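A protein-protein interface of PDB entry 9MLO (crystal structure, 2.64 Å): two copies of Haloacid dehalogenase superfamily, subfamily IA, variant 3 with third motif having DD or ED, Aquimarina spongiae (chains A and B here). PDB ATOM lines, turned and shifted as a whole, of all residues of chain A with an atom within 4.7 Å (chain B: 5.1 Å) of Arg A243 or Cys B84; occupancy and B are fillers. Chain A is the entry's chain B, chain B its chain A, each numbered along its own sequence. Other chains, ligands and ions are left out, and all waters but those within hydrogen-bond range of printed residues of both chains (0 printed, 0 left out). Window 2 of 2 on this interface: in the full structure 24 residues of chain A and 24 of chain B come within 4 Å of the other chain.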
ATOM      1  N   TYR A 239      25.508  13.308   0.492  1.00  0.00           N
ATOM      2  CA  TYR A 239      24.432  13.316   1.478  1.00  0.00           C
ATOM      3  C   TYR A 239      23.782  14.688   1.539  1.00  0.00           C
ATOM      4  O   TYR A 239      22.558  14.806   1.444  1.00  0.00           O
ATOM      5  CB  TYR A 239      24.921  12.905   2.884  1.00  0.00           C
ATOM      6  CG  TYR A 239      23.810  13.103   3.920  1.00  0.00           C
ATOM      7  CD1 TYR A 239      22.877  12.105   4.166  1.00  0.00           C
ATOM      8  CD2 TYR A 239      23.662  14.313   4.593  1.00  0.00           C
ATOM      9  CE1 TYR A 239      21.829  12.292   5.065  1.00  0.00           C
ATOM     10  CE2 TYR A 239      22.624  14.520   5.484  1.00  0.00           C
ATOM     11  CZ  TYR A 239      21.702  13.501   5.725  1.00  0.00           C
ATOM     12  OH  TYR A 239      20.664  13.700   6.625  1.00  0.00           O
ATOM     13  N   LEU A 240      24.593  15.736   1.728  1.00  0.00           N
ATOM     14  CA  LEU A 240      24.033  17.074   1.898  1.00  0.00           C
ATOM     15  C   LEU A 240      23.322  17.533   0.629  1.00  0.00           C
ATOM     16  O   LEU A 240      22.263  18.169   0.697  1.00  0.00           O
ATOM     17  CB  LEU A 240      25.130  18.052   2.306  1.00  0.00           C
ATOM     18  CG  LEU A 240      24.670  19.465   2.660  1.00  0.00           C
ATOM     19  CD1 LEU A 240      23.606  19.426   3.724  1.00  0.00           C
ATOM     20  CD2 LEU A 240      25.833  20.314   3.124  1.00  0.00           C
ATOM     21  N   ASN A 241      23.867  17.166  -0.536  1.00  0.00           N
ATOM     22  CA  ASN A 241      23.282  17.553  -1.817  1.00  0.00           C
ATOM     23  C   ASN A 241      21.904  16.934  -2.023  1.00  0.00           C
ATOM     24  O   ASN A 241      20.944  17.645  -2.340  1.00  0.00           O
ATOM     25  CB  ASN A 241      24.215  17.169  -2.962  1.00  0.00           C
ATOM     26  CG  ASN A 241      25.370  18.123  -3.107  1.00  0.00           C
ATOM     27  OD1 ASN A 241      25.368  19.212  -2.518  1.00  0.00           O
ATOM     28  ND2 ASN A 241      26.369  17.730  -3.901  1.00  0.00           N
ATOM     29  N   LEU A 242      21.779  15.613  -1.877  1.00  0.00           N
ATOM     30  CA  LEU A 242      20.449  15.026  -2.025  1.00  0.00           C
ATOM     31  C   LEU A 242      19.484  15.634  -1.016  1.00  0.00           C
ATOM     32  O   LEU A 242      18.351  15.973  -1.367  1.00  0.00           O
ATOM     33  CB  LEU A 242      20.492  13.502  -1.898  1.00  0.00           C
ATOM     34  N   ARG A 243      19.934  15.846   0.224  1.00  0.00           N
ATOM     35  CA  ARG A 243      19.027  16.347   1.258  1.00  0.00           C
ATOM     36  C   ARG A 243      18.485  17.735   0.920  1.00  0.00           C
ATOM     37  O   ARG A 243      17.309  18.016   1.148  1.00  0.00           O
ATOM     38  CB  ARG A 243      19.725  16.366   2.628  1.00  0.00           C
ATOM     39  CG  ARG A 243      19.893  14.994   3.288  1.00  0.00           C
ATOM     40  CD  ARG A 243      18.571  14.364   3.703  1.00  0.00           C
ATOM     41  NE  ARG A 243      17.785  15.254   4.545  1.00  0.00           N
ATOM     42  CZ  ARG A 243      16.571  14.970   4.991  1.00  0.00           C
ATOM     43  NH1 ARG A 243      15.990  13.813   4.711  1.00  0.00           N
ATOM     44  NH2 ARG A 243      15.920  15.868   5.730  1.00  0.00           N
ATOM     45  N   LEU A 244      19.332  18.628   0.411  1.00  0.00           N
ATOM     46  CA  LEU A 244      18.886  19.982   0.112  1.00  0.00           C
ATOM     47  C   LEU A 244      18.231  20.082  -1.258  1.00  0.00           C
ATOM     48  O   LEU A 244      17.586  21.094  -1.550  1.00  0.00           O
ATOM     49  CB  LEU A 244      20.056  20.970   0.211  1.00  0.00           C
ATOM     50  CG  LEU A 244      20.648  21.236   1.605  1.00  0.00           C
ATOM     51  CD1 LEU A 244      21.990  21.951   1.510  1.00  0.00           C
ATOM     52  CD2 LEU A 244      19.682  22.015   2.500  1.00  0.00           C
ATOM     53  N   ARG A 245      18.375  19.062  -2.103  1.00  0.00           N
ATOM     54  CA  ARG A 245      17.576  19.021  -3.319  1.00  0.00           C
ATOM     55  C   ARG A 245      16.168  18.508  -3.028  1.00  0.00           C
ATOM     56  O   ARG A 245      15.205  18.991  -3.624  1.00  0.00           O
ATOM     57  CB  ARG A 245      18.297  18.188  -4.392  1.00  0.00           C
ATOM     58  CG  ARG A 245      19.420  18.959  -5.102  1.00  0.00           C
ATOM     59  CD  ARG A 245      20.429  18.087  -5.843  1.00  0.00           C
ATOM     60  NE  ARG A 245      21.529  18.910  -6.347  1.00  0.00           N
ATOM     61  CZ  ARG A 245      22.751  18.477  -6.661  1.00  0.00           C
ATOM     62  NH1 ARG A 245      23.093  17.204  -6.551  1.00  0.00           N
ATOM     63  NH2 ARG A 245      23.659  19.351  -7.087  1.00  0.00           N
ATOM     64  N   LYS A 246      16.021  17.578  -2.087  1.00  0.00           N
ATOM     65  CA  LYS A 246      14.688  17.203  -1.636  1.00  0.00           C
ATOM     66  C   LYS A 246      14.036  18.335  -0.848  1.00  0.00           C
ATOM     67  O   LYS A 246      12.842  18.605  -1.018  1.00  0.00           O
ATOM     68  CB  LYS A 246      14.745  15.919  -0.795  1.00  0.00           C
ATOM     69  N   PHE A 247      14.796  19.012   0.014  1.00  0.00           N
ATOM     70  CA  PHE A 247      14.265  20.074   0.870  1.00  0.00           C
ATOM     71  C   PHE A 247      15.142  21.316   0.812  1.00  0.00           C
ATOM     72  O   PHE A 247      16.051  21.480   1.635  1.00  0.00           O
ATOM     73  CB  PHE A 247      14.162  19.622   2.317  1.00  0.00           C
ATOM     74  CG  PHE A 247      13.430  18.346   2.513  1.00  0.00           C
ATOM     75  CD1 PHE A 247      12.045  18.334   2.591  1.00  0.00           C
ATOM     76  CD2 PHE A 247      14.128  17.161   2.666  1.00  0.00           C
ATOM     77  CE1 PHE A 247      11.369  17.145   2.795  1.00  0.00           C
ATOM     78  CE2 PHE A 247      13.453  15.978   2.868  1.00  0.00           C
ATOM     79  CZ  PHE A 247      12.074  15.968   2.939  1.00  0.00           C
ATOM     80  N   LYS A 251      15.373  21.576   6.525  1.00  0.00           N
ATOM     81  CA  LYS A 251      14.532  20.936   7.525  1.00  0.00           C
ATOM     82  C   LYS A 251      14.893  21.408   8.925  1.00  0.00           C
ATOM     83  O   LYS A 251      15.954  21.997   9.142  1.00  0.00           O
ATOM     84  CB  LYS A 251      14.658  19.422   7.426  1.00  0.00           C
ATOM     85  CG  LYS A 251      13.691  18.799   6.448  1.00  0.00           C
ATOM     86  CD  LYS A 251      12.582  18.081   7.193  1.00  0.00           C
ATOM     87  CE  LYS A 251      11.484  17.607   6.267  1.00  0.00           C
ATOM     88  NZ  LYS A 251      10.769  18.766   5.635  1.00  0.00           N
ATOM     89  N   PHE A 253      14.249  20.355  13.279  1.00  0.00           N
ATOM     90  CA  PHE A 253      13.702  19.421  14.252  1.00  0.00           C
ATOM     91  C   PHE A 253      13.768  20.042  15.631  1.00  0.00           C
ATOM     92  O   PHE A 253      14.756  20.699  15.978  1.00  0.00           O
ATOM     93  CB  PHE A 253      14.435  18.089  14.209  1.00  0.00           C
ATOM     94  CG  PHE A 253      14.126  17.304  12.984  1.00  0.00           C
ATOM     95  CD1 PHE A 253      14.689  17.654  11.759  1.00  0.00           C
ATOM     96  CD2 PHE A 253      13.234  16.241  13.032  1.00  0.00           C
ATOM     97  CE1 PHE A 253      14.386  16.934  10.598  1.00  0.00           C
ATOM     98  CE2 PHE A 253      12.928  15.516  11.884  1.00  0.00           C
ATOM     99  CZ  PHE A 253      13.503  15.866  10.664  1.00  0.00           C
ATOM    100  N   ARG A 511      20.349  17.358  10.741  1.00  0.00           N
ATOM    101  CA  ARG A 511      21.513  16.707  10.156  1.00  0.00           C
ATOM    102  C   ARG A 511      22.110  17.559   9.052  1.00  0.00           C
ATOM    103  O   ARG A 511      23.292  17.418   8.728  1.00  0.00           O
ATOM    104  CB  ARG A 511      21.135  15.330   9.605  1.00  0.00           C
ATOM    105  CG  ARG A 511      20.841  14.295  10.662  1.00  0.00           C
ATOM    106  CD  ARG A 511      20.680  12.939  10.036  1.00  0.00           C
ATOM    107  NE  ARG A 511      21.964  12.376   9.660  1.00  0.00           N
ATOM    108  CZ  ARG A 511      22.132  11.309   8.889  1.00  0.00           C
ATOM    109  NH1 ARG A 511      21.117  10.720   8.282  1.00  0.00           N
ATOM    110  NH2 ARG A 511      23.352  10.820   8.723  1.00  0.00           N
ATOM    111  N   GLU A 512      21.305  18.438   8.457  1.00  0.00           N
ATOM    112  CA  GLU A 512      21.805  19.321   7.412  1.00  0.00           C
ATOM    113  C   GLU A 512      22.770  20.354   7.983  1.00  0.00           C
ATOM    114  O   GLU A 512      23.820  20.631   7.388  1.00  0.00           O
ATOM    115  CB  GLU A 512      20.624  20.005   6.714  1.00  0.00           C
ATOM    116  CG  GLU A 512      19.861  19.130   5.698  1.00  0.00           C
ATOM    117  CD  GLU A 512      18.749  18.265   6.312  1.00  0.00           C
ATOM    118  OE1 GLU A 512      18.680  18.106   7.560  1.00  0.00           O
ATOM    119  OE2 GLU A 512      17.927  17.750   5.526  1.00  0.00           O
ATOM    120  N   THR B  80      16.862   8.340  15.744  1.00  0.00           N
ATOM    121  CA  THR B  80      16.732   9.772  15.511  1.00  0.00           C
ATOM    122  C   THR B  80      17.177  10.135  14.098  1.00  0.00           C
ATOM    123  O   THR B  80      16.533  10.950  13.426  1.00  0.00           O
ATOM    124  CB  THR B  80      17.524  10.553  16.562  1.00  0.00           C
ATOM    125  OG1 THR B  80      16.861  10.436  17.823  1.00  0.00           O
ATOM    126  CG2 THR B  80      17.598  12.029  16.202  1.00  0.00           C
ATOM    127  N   ALA B  81      18.255   9.515  13.620  1.00  0.00           N
ATOM    128  CA  ALA B  81      18.682   9.747  12.247  1.00  0.00           C
ATOM    129  C   ALA B  81      17.652   9.200  11.256  1.00  0.00           C
ATOM    130  O   ALA B  81      17.263   9.888  10.305  1.00  0.00           O
ATOM    131  CB  ALA B  81      20.068   9.128  12.032  1.00  0.00           C
ATOM    132  N   LEU B  82      17.174   7.971  11.479  1.00  0.00           N
ATOM    133  CA  LEU B  82      16.243   7.354  10.537  1.00  0.00           C
ATOM    134  C   LEU B  82      14.915   8.097  10.482  1.00  0.00           C
ATOM    135  O   LEU B  82      14.235   8.044   9.455  1.00  0.00           O
ATOM    136  CB  LEU B  82      16.028   5.885  10.897  1.00  0.00           C
ATOM    137  CG  LEU B  82      17.245   5.001  10.614  1.00  0.00           C
ATOM    138  CD1 LEU B  82      17.065   3.625  11.191  1.00  0.00           C
ATOM    139  CD2 LEU B  82      17.514   4.919   9.120  1.00  0.00           C
ATOM    140  N   SER B  83      14.526   8.784  11.563  1.00  0.00           N
ATOM    141  CA  SER B  83      13.362   9.666  11.497  1.00  0.00           C
ATOM    142  C   SER B  83      13.511  10.657  10.368  1.00  0.00           C
ATOM    143  O   SER B  83      12.588  10.870   9.576  1.00  0.00           O
ATOM    144  CB  SER B  83      13.187  10.437  12.793  1.00  0.00           C
ATOM    145  OG  SER B  83      12.842   9.566  13.821  1.00  0.00           O
ATOM    146  N   CYS B  84      14.674  11.301  10.307  1.00  0.00           N
ATOM    147  CA  CYS B  84      14.967  12.217   9.215  1.00  0.00           C
ATOM    148  C   CYS B  84      14.933  11.493   7.871  1.00  0.00           C
ATOM    149  O   CYS B  84      14.208  11.887   6.951  1.00  0.00           O
ATOM    150  CB  CYS B  84      16.329  12.860   9.436  1.00  0.00           C
ATOM    151  SG  CYS B  84      16.558  14.319   8.452  1.00  0.00           S
ATOM    152  N   GLU B  85      15.706  10.415   7.750  1.00  0.00           N
ATOM    153  CA  GLU B  85      15.874   9.790   6.448  1.00  0.00           C
ATOM    154  C   GLU B  85      14.594   9.110   5.975  1.00  0.00           C
ATOM    155  O   GLU B  85      14.273   9.153   4.782  1.00  0.00           O
ATOM    156  CB  GLU B  85      17.040   8.804   6.489  1.00  0.00           C
ATOM    157  CG  GLU B  85      18.371   9.457   6.823  1.00  0.00           C
ATOM    158  CD  GLU B  85      18.533  10.836   6.203  1.00  0.00           C
ATOM    159  OE1 GLU B  85      18.389  10.966   4.964  1.00  0.00           O
ATOM    160  OE2 GLU B  85      18.798  11.798   6.963  1.00  0.00           O
ATOM    161  N   LEU B  86      13.850   8.485   6.879  1.00  0.00           N
ATOM    162  CA  LEU B  86      12.643   7.767   6.501  1.00  0.00           C
ATOM    163  C   LEU B  86      11.375   8.606   6.656  1.00  0.00           C
ATOM    164  O   LEU B  86      10.278   8.112   6.368  1.00  0.00           O
ATOM    165  CB  LEU B  86      12.531   6.467   7.308  1.00  0.00           C
ATOM    166  CG  LEU B  86      13.674   5.448   7.192  1.00  0.00           C
ATOM    167  CD1 LEU B  86      13.306   4.161   7.893  1.00  0.00           C
ATOM    168  CD2 LEU B  86      14.068   5.165   5.769  1.00  0.00           C
ATOM    169  N   GLU B  87      11.500   9.867   7.072  1.00  0.00           N
ATOM    170  CA  GLU B  87      10.364  10.788   7.174  1.00  0.00           C
ATOM    171  C   GLU B  87       9.256  10.210   8.053  1.00  0.00           C
ATOM    172  O   GLU B  87       8.062  10.368   7.787  1.00  0.00           O
ATOM    173  CB  GLU B  87       9.841  11.161   5.784  1.00  0.00           C
ATOM    174  CG  GLU B  87      10.964  11.284   4.754  1.00  0.00           C
ATOM    175  CD  GLU B  87      10.641  12.232   3.618  1.00  0.00           C
ATOM    176  OE1 GLU B  87       9.693  13.023   3.774  1.00  0.00           O
ATOM    177  OE2 GLU B  87      11.339  12.192   2.575  1.00  0.00           O
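Arg A243 touches two residues of chain B. Of chain A, only Arg A243 comes within 4 Å of Cys B84. Of the printed residues of chain B, Phe A247 touches Glu B87 (3.9 Å). Of the printed residues of chain B, Tyr A239 touches Glu B85. Printed residues of chain A within 4 Å of Glu B85: Tyr A239 (2.7 Å), Arg A243 (3.6 Å) and Arg A511 (2.9 Å). Ala B81 touches none of the printed residues of chain A. Leu A244 touches none of the printed residues of chain B. The nearest printed residue of chain B that does not touch Arg A511 is Ala B81 (4.2 Å).
Of the 8 printed residues of chain B, 3 touch a printed residue of chain A. Printed residues of chain B that touch a printed residue of chain A: Cys B84, Glu B85 and Glu B87.
NE of Arg A243 lies within salt-bridge range of OE2 of Glu A512. The side-chain sulfur of Cys B84 lies close to the side-chain carboxylate of Glu B85. The side-chain hydroxyl of Tyr A239 sits close to the guanidinium group of Arg A511, at 3.4 Å.
Among the printed residues, pairs that only touch across the chains: Phe A247 with Glu B87.
NH1 of Arg A511 lies within salt-bridge range of OE2 of Glu B85, 2.9 Å away. The side-chain carboxylate (OE1) of Glu B85 lies within salt-bridge range of the guanidinium group (NH1) of Arg A243, at 3.7 Å. The side-chain sulfur (SG) of Cys B84 lies within hydrogen-bond range of the guanidinium group (NH2) of Arg A243, 3.2 Å away. The side-chain carboxylate of Glu B85 lies within hydrogen-bond range of the side-chain hydroxyl of Tyr A239 (2.7 Å).
No position is printed for both chains.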
